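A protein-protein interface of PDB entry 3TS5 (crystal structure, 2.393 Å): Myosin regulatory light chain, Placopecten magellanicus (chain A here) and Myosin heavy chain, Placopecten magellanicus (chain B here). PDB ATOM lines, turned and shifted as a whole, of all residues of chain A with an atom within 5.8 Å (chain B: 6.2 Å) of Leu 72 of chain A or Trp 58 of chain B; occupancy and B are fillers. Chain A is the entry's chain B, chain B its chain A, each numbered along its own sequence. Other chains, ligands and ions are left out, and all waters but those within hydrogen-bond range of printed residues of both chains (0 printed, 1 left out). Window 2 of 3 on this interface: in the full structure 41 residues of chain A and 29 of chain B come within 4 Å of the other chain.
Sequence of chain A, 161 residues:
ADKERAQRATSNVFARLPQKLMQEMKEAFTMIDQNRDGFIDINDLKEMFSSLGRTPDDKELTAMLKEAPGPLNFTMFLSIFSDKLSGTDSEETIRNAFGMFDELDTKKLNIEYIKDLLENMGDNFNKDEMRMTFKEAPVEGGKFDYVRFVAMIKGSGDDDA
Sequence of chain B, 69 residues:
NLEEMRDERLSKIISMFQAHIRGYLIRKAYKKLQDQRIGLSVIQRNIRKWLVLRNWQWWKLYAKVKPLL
The indole nitrogen of Trp 58 of chain B is in hydrogen-bond range of the backbone carbonyl oxygen of Met 64 of chain A (2.9 Å). NE1 of Trp 56 of chain B is in hydrogen-bond range of OE1 of Glu 67 of chain A (2.7 Å).
The backbone NH (N) of Ile 40 of chain A lies within hydrogen-bond range of the backbone carbonyl oxygen (O) of Leu 72 of chain A (2.9 Å).
Leu 45 of chain A touches Trp 58 of chain B. Leu 45 of chain A touches Leu 61 of chain B (CD1 to CD2, 3.99 Å). Met 64 of chain A touches Gln 57 of chain B (SD to CG, 3.4 Å). Glu 67 of chain A touches Trp 58 of chain B (OE2 to CD1, 3.4 Å). Leu 72 of chain A touches Trp 58 of chain B (CD1 to CH2, 3.6 Å). Trp 56 of chain B touches Ile 80 of chain A. Phe 81 of chain A touches Trp 56 of chain B (CE1 to CZ3, 3.8 Å). Phe 81 of chain A touches Trp 58 of chain B. Phe 81 of chain A touches Tyr 62 of chain B (CE1 to CD1, 3.7 Å).
Leu 72 of chain A touches one residue of chain B. Of the printed residues of chain A, Trp 58 of chain B touches Leu 45 (3.98 Å), Met 64 (2.9 Å), Glu 67 (3.4 Å), Leu 72 (3.6 Å) and Phe 81 (3.7 Å). Printed residues of chain B within 4 Å of Leu 45 of chain A: Trp 58 and Leu 61. Printed residues of chain A within 4 Å of Gln 57 of chain B: Met 64. The nearest printed residue of chain A that does not touch Tyr 62 of chain B is Phe 77 of chain A (4.4 Å).
Hydrophobic or aromatic side chains of chain A within 4 Å of the printed part of chain B: Leu 45, Met 64, Leu 72, Ile 80 and Phe 81. Hydrophobic or aromatic side chains of chain B that line the printed part of chain A: Trp 56, Trp 58, Leu 61 and Tyr 62. Among the printed residues, no Asp or Glu carboxylate lies within 4 Å of a Lys or Arg side-chain nitrogen of the other chain.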
ATOM      1  N   PHE A  29       4.951 -19.536   3.560  1.00  0.00           N
ATOM      2  CA  PHE A  29       6.390 -19.721   3.607  1.00  0.00           C
ATOM      3  C   PHE A  29       6.774 -20.495   4.869  1.00  0.00           C
ATOM      4  O   PHE A  29       7.577 -21.446   4.830  1.00  0.00           O
ATOM      5  CB  PHE A  29       7.120 -18.372   3.566  1.00  0.00           C
ATOM      6  CG  PHE A  29       8.610 -18.506   3.696  1.00  0.00           C
ATOM      7  CD1 PHE A  29       9.408 -18.671   2.570  1.00  0.00           C
ATOM      8  CD2 PHE A  29       9.215 -18.526   4.951  1.00  0.00           C
ATOM      9  CE1 PHE A  29      10.778 -18.831   2.688  1.00  0.00           C
ATOM     10  CE2 PHE A  29      10.589 -18.682   5.071  1.00  0.00           C
ATOM     11  CZ  PHE A  29      11.371 -18.832   3.932  1.00  0.00           C
ATOM     12  N   ILE A  32       5.944 -24.256   4.671  1.00  0.00           N
ATOM     13  CA  ILE A  32       6.785 -24.997   3.737  1.00  0.00           C
ATOM     14  C   ILE A  32       8.189 -25.180   4.304  1.00  0.00           C
ATOM     15  O   ILE A  32       8.819 -26.209   4.087  1.00  0.00           O
ATOM     16  CB  ILE A  32       6.843 -24.326   2.355  1.00  0.00           C
ATOM     17  CG1 ILE A  32       5.463 -24.346   1.717  1.00  0.00           C
ATOM     18  CG2 ILE A  32       7.814 -25.057   1.450  1.00  0.00           C
ATOM     19  CD1 ILE A  32       5.338 -23.428   0.557  1.00  0.00           C
ATOM     20  N   GLY A  38      14.259 -20.702   8.011  1.00  0.00           N
ATOM     21  CA  GLY A  38      14.154 -19.397   7.371  1.00  0.00           C
ATOM     22  C   GLY A  38      14.507 -19.459   5.884  1.00  0.00           C
ATOM     23  O   GLY A  38      14.603 -18.437   5.212  1.00  0.00           O
ATOM     24  N   PHE A  39      14.712 -20.673   5.378  1.00  0.00           N
ATOM     25  CA  PHE A  39      14.934 -20.906   3.954  1.00  0.00           C
ATOM     26  C   PHE A  39      14.071 -22.057   3.506  1.00  0.00           C
ATOM     27  O   PHE A  39      13.820 -22.972   4.261  1.00  0.00           O
ATOM     28  CB  PHE A  39      16.404 -21.247   3.658  1.00  0.00           C
ATOM     29  CG  PHE A  39      17.343 -20.117   3.936  1.00  0.00           C
ATOM     30  CD1 PHE A  39      17.537 -19.116   2.996  1.00  0.00           C
ATOM     31  CD2 PHE A  39      18.015 -20.038   5.151  1.00  0.00           C
ATOM     32  CE1 PHE A  39      18.392 -18.051   3.257  1.00  0.00           C
ATOM     33  CE2 PHE A  39      18.869 -18.979   5.419  1.00  0.00           C
ATOM     34  CZ  PHE A  39      19.060 -17.984   4.472  1.00  0.00           C
ATOM     35  N   ILE A  40      13.606 -22.016   2.273  1.00  0.00           N
ATOM     36  CA  ILE A  40      13.027 -23.214   1.705  1.00  0.00           C
ATOM     37  C   ILE A  40      14.048 -23.870   0.790  1.00  0.00           C
ATOM     38  O   ILE A  40      14.508 -23.257  -0.191  1.00  0.00           O
ATOM     39  CB  ILE A  40      11.712 -22.929   0.951  1.00  0.00           C
ATOM     40  CG1 ILE A  40      10.637 -22.432   1.935  1.00  0.00           C
ATOM     41  CG2 ILE A  40      11.252 -24.196   0.210  1.00  0.00           C
ATOM     42  CD1 ILE A  40       9.408 -21.852   1.258  1.00  0.00           C
ATOM     43  N   ASP A  41      14.418 -25.106   1.113  1.00  0.00           N
ATOM     44  CA  ASP A  41      15.271 -25.891   0.210  1.00  0.00           C
ATOM     45  C   ASP A  41      14.548 -27.122  -0.316  1.00  0.00           C
ATOM     46  O   ASP A  41      13.340 -27.279  -0.116  1.00  0.00           O
ATOM     47  CB  ASP A  41      16.600 -26.273   0.868  1.00  0.00           C
ATOM     48  CG  ASP A  41      16.439 -27.283   2.010  1.00  0.00           C
ATOM     49  OD1 ASP A  41      15.309 -27.751   2.285  1.00  0.00           O
ATOM     50  OD2 ASP A  41      17.472 -27.614   2.636  1.00  0.00           O
ATOM     51  N   LEU A  45      10.715 -28.796   0.383  1.00  0.00           N
ATOM     52  CA  LEU A  45       9.792 -28.984  -0.734  1.00  0.00           C
ATOM     53  C   LEU A  45       9.316 -30.429  -0.847  1.00  0.00           C
ATOM     54  O   LEU A  45       8.105 -30.672  -0.979  1.00  0.00           O
ATOM     55  CB  LEU A  45      10.468 -28.545  -2.040  1.00  0.00           C
ATOM     56  CG  LEU A  45       9.816 -27.457  -2.888  1.00  0.00           C
ATOM     57  CD1 LEU A  45       9.144 -26.403  -2.020  1.00  0.00           C
ATOM     58  CD2 LEU A  45      10.837 -26.834  -3.830  1.00  0.00           C
ATOM     59  N   ALA A  63      14.154 -27.237 -10.310  1.00  0.00           N
ATOM     60  CA  ALA A  63      13.726 -26.209 -11.240  1.00  0.00           C
ATOM     61  C   ALA A  63      12.868 -25.133 -10.540  1.00  0.00           C
ATOM     62  O   ALA A  63      13.053 -23.934 -10.795  1.00  0.00           O
ATOM     63  CB  ALA A  63      12.997 -26.827 -12.432  1.00  0.00           C
ATOM     64  N   MET A  64      11.954 -25.548  -9.653  1.00  0.00           N
ATOM     65  CA  MET A  64      11.170 -24.581  -8.866  1.00  0.00           C
ATOM     66  C   MET A  64      12.086 -23.684  -8.069  1.00  0.00           C
ATOM     67  O   MET A  64      11.879 -22.480  -8.001  1.00  0.00           O
ATOM     68  CB  MET A  64      10.206 -25.256  -7.900  1.00  0.00           C
ATOM     69  CG  MET A  64       9.040 -25.971  -8.543  1.00  0.00           C
ATOM     70  SD  MET A  64       7.966 -26.801  -7.325  1.00  0.00           S
ATOM     71  CE  MET A  64       7.404 -25.379  -6.366  1.00  0.00           C
ATOM     72  N   LEU A  65      13.104 -24.279  -7.459  1.00  0.00           N
ATOM     73  CA  LEU A  65      14.066 -23.521  -6.659  1.00  0.00           C
ATOM     74  C   LEU A  65      14.924 -22.561  -7.519  1.00  0.00           C
ATOM     75  O   LEU A  65      15.239 -21.438  -7.092  1.00  0.00           O
ATOM     76  CB  LEU A  65      14.926 -24.481  -5.826  1.00  0.00           C
ATOM     77  CG  LEU A  65      14.122 -25.275  -4.788  1.00  0.00           C
ATOM     78  CD1 LEU A  65      14.988 -26.301  -4.023  1.00  0.00           C
ATOM     79  CD2 LEU A  65      13.401 -24.340  -3.796  1.00  0.00           C
ATOM     80  N   GLU A  67      13.957 -20.842  -9.963  1.00  0.00           N
ATOM     81  CA  GLU A  67      13.195 -19.625 -10.275  1.00  0.00           C
ATOM     82  C   GLU A  67      13.576 -18.491  -9.344  1.00  0.00           C
ATOM     83  O   GLU A  67      13.259 -17.336  -9.604  1.00  0.00           O
ATOM     84  CB  GLU A  67      11.682 -19.865 -10.201  1.00  0.00           C
ATOM     85  CG  GLU A  67      11.139 -20.788 -11.274  1.00  0.00           C
ATOM     86  CD  GLU A  67       9.638 -21.040 -11.121  1.00  0.00           C
ATOM     87  OE1 GLU A  67       8.863 -20.050 -11.074  1.00  0.00           O
ATOM     88  OE2 GLU A  67       9.233 -22.229 -11.045  1.00  0.00           O
ATOM     89  N   ALA A  68      14.256 -18.833  -8.252  1.00  0.00           N
ATOM     90  CA  ALA A  68      14.749 -17.840  -7.305  1.00  0.00           C
ATOM     91  C   ALA A  68      16.225 -17.530  -7.567  1.00  0.00           C
ATOM     92  O   ALA A  68      17.055 -18.432  -7.575  1.00  0.00           O
ATOM     93  CB  ALA A  68      14.557 -18.337  -5.872  1.00  0.00           C
ATOM     94  N   GLY A  70      18.507 -16.229  -5.667  1.00  0.00           N
ATOM     95  CA  GLY A  70      19.332 -16.782  -4.604  1.00  0.00           C
ATOM     96  C   GLY A  70      18.602 -17.730  -3.658  1.00  0.00           C
ATOM     97  O   GLY A  70      17.485 -18.169  -3.956  1.00  0.00           O
ATOM     98  N   PRO A  71      19.234 -18.052  -2.509  1.00  0.00           N
ATOM     99  CA  PRO A  71      18.656 -18.885  -1.436  1.00  0.00           C
ATOM    100  C   PRO A  71      17.257 -18.407  -1.069  1.00  0.00           C
ATOM    101  O   PRO A  71      17.039 -17.199  -0.935  1.00  0.00           O
ATOM    102  CB  PRO A  71      19.605 -18.655  -0.257  1.00  0.00           C
ATOM    103  CG  PRO A  71      20.929 -18.351  -0.910  1.00  0.00           C
ATOM    104  CD  PRO A  71      20.589 -17.575  -2.171  1.00  0.00           C
ATOM    105  N   LEU A  72      16.333 -19.349  -0.909  1.00  0.00           N
ATOM    106  CA  LEU A  72      14.919 -19.021  -0.754  1.00  0.00           C
ATOM    107  C   LEU A  72      14.523 -18.552   0.642  1.00  0.00           C
ATOM    108  O   LEU A  72      13.834 -19.251   1.377  1.00  0.00           O
ATOM    109  CB  LEU A  72      14.042 -20.182  -1.203  1.00  0.00           C
ATOM    110  CG  LEU A  72      12.992 -19.843  -2.253  1.00  0.00           C
ATOM    111  CD1 LEU A  72      12.111 -21.056  -2.538  1.00  0.00           C
ATOM    112  CD2 LEU A  72      12.150 -18.663  -1.791  1.00  0.00           C
ATOM    113  N   ASN A  73      14.974 -17.344   0.957  1.00  0.00           N
ATOM    114  CA  ASN A  73      14.525 -16.590   2.106  1.00  0.00           C
ATOM    115  C   ASN A  73      13.053 -16.294   1.922  1.00  0.00           C
ATOM    116  O   ASN A  73      12.483 -16.573   0.873  1.00  0.00           O
ATOM    117  CB  ASN A  73      15.268 -15.255   2.154  1.00  0.00           C
ATOM    118  CG  ASN A  73      16.390 -15.242   3.163  1.00  0.00           C
ATOM    119  OD1 ASN A  73      16.342 -15.936   4.175  1.00  0.00           O
ATOM    120  ND2 ASN A  73      17.411 -14.439   2.894  1.00  0.00           N
ATOM    121  N   PHE A  74      12.442 -15.703   2.936  1.00  0.00           N
ATOM    122  CA  PHE A  74      11.093 -15.190   2.794  1.00  0.00           C
ATOM    123  C   PHE A  74      11.077 -13.995   1.833  1.00  0.00           C
ATOM    124  O   PHE A  74      10.114 -13.801   1.098  1.00  0.00           O
ATOM    125  CB  PHE A  74      10.448 -14.798   4.129  1.00  0.00           C
ATOM    126  CG  PHE A  74       9.107 -14.130   3.958  1.00  0.00           C
ATOM    127  CD1 PHE A  74       8.018 -14.846   3.479  1.00  0.00           C
ATOM    128  CD2 PHE A  74       8.945 -12.772   4.211  1.00  0.00           C
ATOM    129  CE1 PHE A  74       6.786 -14.229   3.291  1.00  0.00           C
ATOM    130  CE2 PHE A  74       7.712 -12.157   4.025  1.00  0.00           C
ATOM    131  CZ  PHE A  74       6.637 -12.886   3.567  1.00  0.00           C
ATOM    132  N   MET A  76      13.032 -13.568  -0.738  1.00  0.00           N
ATOM    133  CA  MET A  76      13.105 -14.189  -2.049  1.00  0.00           C
ATOM    134  C   MET A  76      11.741 -14.808  -2.415  1.00  0.00           C
ATOM    135  O   MET A  76      11.317 -14.786  -3.567  1.00  0.00           O
ATOM    136  CB  MET A  76      14.198 -15.263  -2.042  1.00  0.00           C
ATOM    137  CG  MET A  76      14.512 -15.872  -3.400  1.00  0.00           C
ATOM    138  SD  MET A  76      15.053 -14.648  -4.628  1.00  0.00           S
ATOM    139  CE  MET A  76      16.490 -13.936  -3.817  1.00  0.00           C
ATOM    140  N   PHE A  77      11.061 -15.365  -1.423  1.00  0.00           N
ATOM    141  CA  PHE A  77       9.765 -16.001  -1.640  1.00  0.00           C
ATOM    142  C   PHE A  77       8.780 -14.942  -2.109  1.00  0.00           C
ATOM    143  O   PHE A  77       7.983 -15.162  -3.015  1.00  0.00           O
ATOM    144  CB  PHE A  77       9.315 -16.621  -0.315  1.00  0.00           C
ATOM    145  CG  PHE A  77       7.989 -17.326  -0.356  1.00  0.00           C
ATOM    146  CD1 PHE A  77       7.910 -18.664  -0.713  1.00  0.00           C
ATOM    147  CD2 PHE A  77       6.832 -16.676   0.034  1.00  0.00           C
ATOM    148  CE1 PHE A  77       6.692 -19.343  -0.708  1.00  0.00           C
ATOM    149  CE2 PHE A  77       5.609 -17.346   0.044  1.00  0.00           C
ATOM    150  CZ  PHE A  77       5.543 -18.684  -0.319  1.00  0.00           C
ATOM    151  N   ILE A  80       9.173 -13.973  -5.643  1.00  0.00           N
ATOM    152  CA  ILE A  80       8.643 -14.998  -6.543  1.00  0.00           C
ATOM    153  C   ILE A  80       7.108 -14.946  -6.679  1.00  0.00           C
ATOM    154  O   ILE A  80       6.554 -15.275  -7.736  1.00  0.00           O
ATOM    155  CB  ILE A  80       9.105 -16.392  -6.101  1.00  0.00           C
ATOM    156  CG1 ILE A  80      10.506 -16.674  -6.629  1.00  0.00           C
ATOM    157  CG2 ILE A  80       8.148 -17.490  -6.565  1.00  0.00           C
ATOM    158  CD1 ILE A  80      10.918 -18.136  -6.405  1.00  0.00           C
ATOM    159  N   PHE A  81       6.426 -14.514  -5.622  1.00  0.00           N
ATOM    160  CA  PHE A  81       4.955 -14.528  -5.624  1.00  0.00           C
ATOM    161  C   PHE A  81       4.275 -13.169  -5.807  1.00  0.00           C
ATOM    162  O   PHE A  81       3.150 -13.109  -6.303  1.00  0.00           O
ATOM    163  CB  PHE A  81       4.397 -15.190  -4.351  1.00  0.00           C
ATOM    164  CG  PHE A  81       4.398 -16.691  -4.397  1.00  0.00           C
ATOM    165  CD1 PHE A  81       3.343 -17.375  -4.969  1.00  0.00           C
ATOM    166  CD2 PHE A  81       5.460 -17.421  -3.861  1.00  0.00           C
ATOM    167  CE1 PHE A  81       3.340 -18.763  -5.011  1.00  0.00           C
ATOM    168  CE2 PHE A  81       5.469 -18.810  -3.904  1.00  0.00           C
ATOM    169  CZ  PHE A  81       4.408 -19.483  -4.479  1.00  0.00           C
ATOM    170  N   TRP B  56       1.455 -22.982 -13.190  1.00  0.00           N
ATOM    171  CA  TRP B  56       2.699 -22.682 -12.498  1.00  0.00           C
ATOM    172  C   TRP B  56       2.757 -23.534 -11.231  1.00  0.00           C
ATOM    173  O   TRP B  56       1.877 -23.450 -10.365  1.00  0.00           O
ATOM    174  CB  TRP B  56       2.745 -21.195 -12.141  1.00  0.00           C
ATOM    175  CG  TRP B  56       4.020 -20.710 -11.535  1.00  0.00           C
ATOM    176  CD1 TRP B  56       5.289 -21.058 -11.893  1.00  0.00           C
ATOM    177  CD2 TRP B  56       4.149 -19.758 -10.477  1.00  0.00           C
ATOM    178  NE1 TRP B  56       6.205 -20.388 -11.116  1.00  0.00           N
ATOM    179  CE2 TRP B  56       5.530 -19.582 -10.238  1.00  0.00           C
ATOM    180  CE3 TRP B  56       3.230 -19.035  -9.701  1.00  0.00           C
ATOM    181  CZ2 TRP B  56       6.018 -18.713  -9.263  1.00  0.00           C
ATOM    182  CZ3 TRP B  56       3.715 -18.186  -8.722  1.00  0.00           C
ATOM    183  CH2 TRP B  56       5.095 -18.029  -8.513  1.00  0.00           C
ATOM    184  N   GLN B  57       3.803 -24.348 -11.141  1.00  0.00           N
ATOM    185  CA  GLN B  57       3.952 -25.324 -10.075  1.00  0.00           C
ATOM    186  C   GLN B  57       3.994 -24.698  -8.674  1.00  0.00           C
ATOM    187  O   GLN B  57       3.436 -25.252  -7.726  1.00  0.00           O
ATOM    188  CB  GLN B  57       5.190 -26.199 -10.334  1.00  0.00           C
ATOM    189  CG  GLN B  57       5.292 -27.414  -9.411  1.00  0.00           C
ATOM    190  CD  GLN B  57       4.084 -28.330  -9.494  1.00  0.00           C
ATOM    191  OE1 GLN B  57       3.275 -28.395  -8.558  1.00  0.00           O
ATOM    192  NE2 GLN B  57       3.950 -29.040 -10.613  1.00  0.00           N
ATOM    193  N   TRP B  58       4.650 -23.549  -8.553  1.00  0.00           N
ATOM    194  CA  TRP B  58       4.654 -22.811  -7.306  1.00  0.00           C
ATOM    195  C   TRP B  58       3.236 -22.510  -6.843  1.00  0.00           C
ATOM    196  O   TRP B  58       2.932 -22.638  -5.660  1.00  0.00           O
ATOM    197  CB  TRP B  58       5.461 -21.512  -7.421  1.00  0.00           C
ATOM    198  CG  TRP B  58       6.908 -21.710  -7.105  1.00  0.00           C
ATOM    199  CD1 TRP B  58       7.956 -21.579  -7.963  1.00  0.00           C
ATOM    200  CD2 TRP B  58       7.473 -22.103  -5.839  1.00  0.00           C
ATOM    201  NE1 TRP B  58       9.136 -21.842  -7.319  1.00  0.00           N
ATOM    202  CE2 TRP B  58       8.875 -22.172  -6.014  1.00  0.00           C
ATOM    203  CE3 TRP B  58       6.929 -22.397  -4.574  1.00  0.00           C
ATOM    204  CZ2 TRP B  58       9.755 -22.527  -4.969  1.00  0.00           C
ATOM    205  CZ3 TRP B  58       7.795 -22.747  -3.537  1.00  0.00           C
ATOM    206  CH2 TRP B  58       9.198 -22.811  -3.743  1.00  0.00           C
ATOM    207  N   TRP B  59       2.370 -22.115  -7.776  1.00  0.00           N
ATOM    208  CA  TRP B  59       1.005 -21.753  -7.400  1.00  0.00           C
ATOM    209  C   TRP B  59       0.185 -22.972  -6.988  1.00  0.00           C
ATOM    210  O   TRP B  59      -0.609 -22.907  -6.045  1.00  0.00           O
ATOM    211  CB  TRP B  59       0.293 -20.984  -8.513  1.00  0.00           C
ATOM    212  CG  TRP B  59      -1.188 -21.215  -8.483  1.00  0.00           C
ATOM    213  CD1 TRP B  59      -1.917 -22.036  -9.311  1.00  0.00           C
ATOM    214  CD2 TRP B  59      -2.126 -20.655  -7.554  1.00  0.00           C
ATOM    215  NE1 TRP B  59      -3.244 -22.002  -8.967  1.00  0.00           N
ATOM    216  CE2 TRP B  59      -3.402 -21.164  -7.893  1.00  0.00           C
ATOM    217  CE3 TRP B  59      -2.009 -19.775  -6.471  1.00  0.00           C
ATOM    218  CZ2 TRP B  59      -4.554 -20.814  -7.193  1.00  0.00           C
ATOM    219  CZ3 TRP B  59      -3.148 -19.425  -5.781  1.00  0.00           C
ATOM    220  CH2 TRP B  59      -4.408 -19.943  -6.143  1.00  0.00           C
ATOM    221  N   LYS B  60       0.371 -24.081  -7.698  1.00  0.00           N
ATOM    222  CA  LYS B  60      -0.373 -25.305  -7.396  1.00  0.00           C
ATOM    223  C   LYS B  60      -0.077 -25.772  -5.974  1.00  0.00           C
ATOM    224  O   LYS B  60      -0.984 -26.176  -5.236  1.00  0.00           O
ATOM    225  CB  LYS B  60      -0.038 -26.407  -8.407  1.00  0.00           C
ATOM    226  CG  LYS B  60      -0.512 -26.104  -9.827  1.00  0.00           C
ATOM    227  CD  LYS B  60       0.116 -27.051 -10.833  1.00  0.00           C
ATOM    228  CE  LYS B  60      -0.754 -27.179 -12.076  1.00  0.00           C
ATOM    229  NZ  LYS B  60      -0.086 -27.994 -13.136  1.00  0.00           N
ATOM    230  N   LEU B  61       1.202 -25.720  -5.610  1.00  0.00           N
ATOM    231  CA  LEU B  61       1.634 -25.930  -4.245  1.00  0.00           C
ATOM    232  C   LEU B  61       0.923 -24.928  -3.329  1.00  0.00           C
ATOM    233  O   LEU B  61       0.188 -25.302  -2.404  1.00  0.00           O
ATOM    234  CB  LEU B  61       3.152 -25.735  -4.133  1.00  0.00           C
ATOM    235  CG  LEU B  61       3.705 -26.004  -2.727  1.00  0.00           C
ATOM    236  CD1 LEU B  61       3.256 -27.376  -2.284  1.00  0.00           C
ATOM    237  CD2 LEU B  61       5.235 -25.873  -2.635  1.00  0.00           C
ATOM    238  N   TYR B  62       1.161 -23.652  -3.597  1.00  0.00           N
ATOM    239  CA  TYR B  62       0.595 -22.595  -2.792  1.00  0.00           C
ATOM    240  C   TYR B  62      -0.905 -22.810  -2.513  1.00  0.00           C
ATOM    241  O   TYR B  62      -1.367 -22.648  -1.383  1.00  0.00           O
ATOM    242  CB  TYR B  62       0.830 -21.253  -3.473  1.00  0.00           C
ATOM    243  CG  TYR B  62       0.495 -20.075  -2.606  1.00  0.00           C
ATOM    244  CD1 TYR B  62       1.477 -19.441  -1.845  1.00  0.00           C
ATOM    245  CD2 TYR B  62      -0.812 -19.578  -2.550  1.00  0.00           C
ATOM    246  CE1 TYR B  62       1.172 -18.335  -1.037  1.00  0.00           C
ATOM    247  CE2 TYR B  62      -1.136 -18.468  -1.746  1.00  0.00           C
ATOM    248  CZ  TYR B  62      -0.136 -17.855  -0.995  1.00  0.00           C
ATOM    249  OH  TYR B  62      -0.442 -16.769  -0.210  1.00  0.00           O
ATOM    250  N   ALA B  63      -1.664 -23.178  -3.539  1.00  0.00           N
ATOM    251  CA  ALA B  63      -3.103 -23.293  -3.371  1.00  0.00           C
ATOM    252  C   ALA B  63      -3.526 -24.535  -2.573  1.00  0.00           C
ATOM    253  O   ALA B  63      -4.626 -24.580  -2.020  1.00  0.00           O
ATOM    254  CB  ALA B  63      -3.783 -23.297  -4.732  1.00  0.00           C
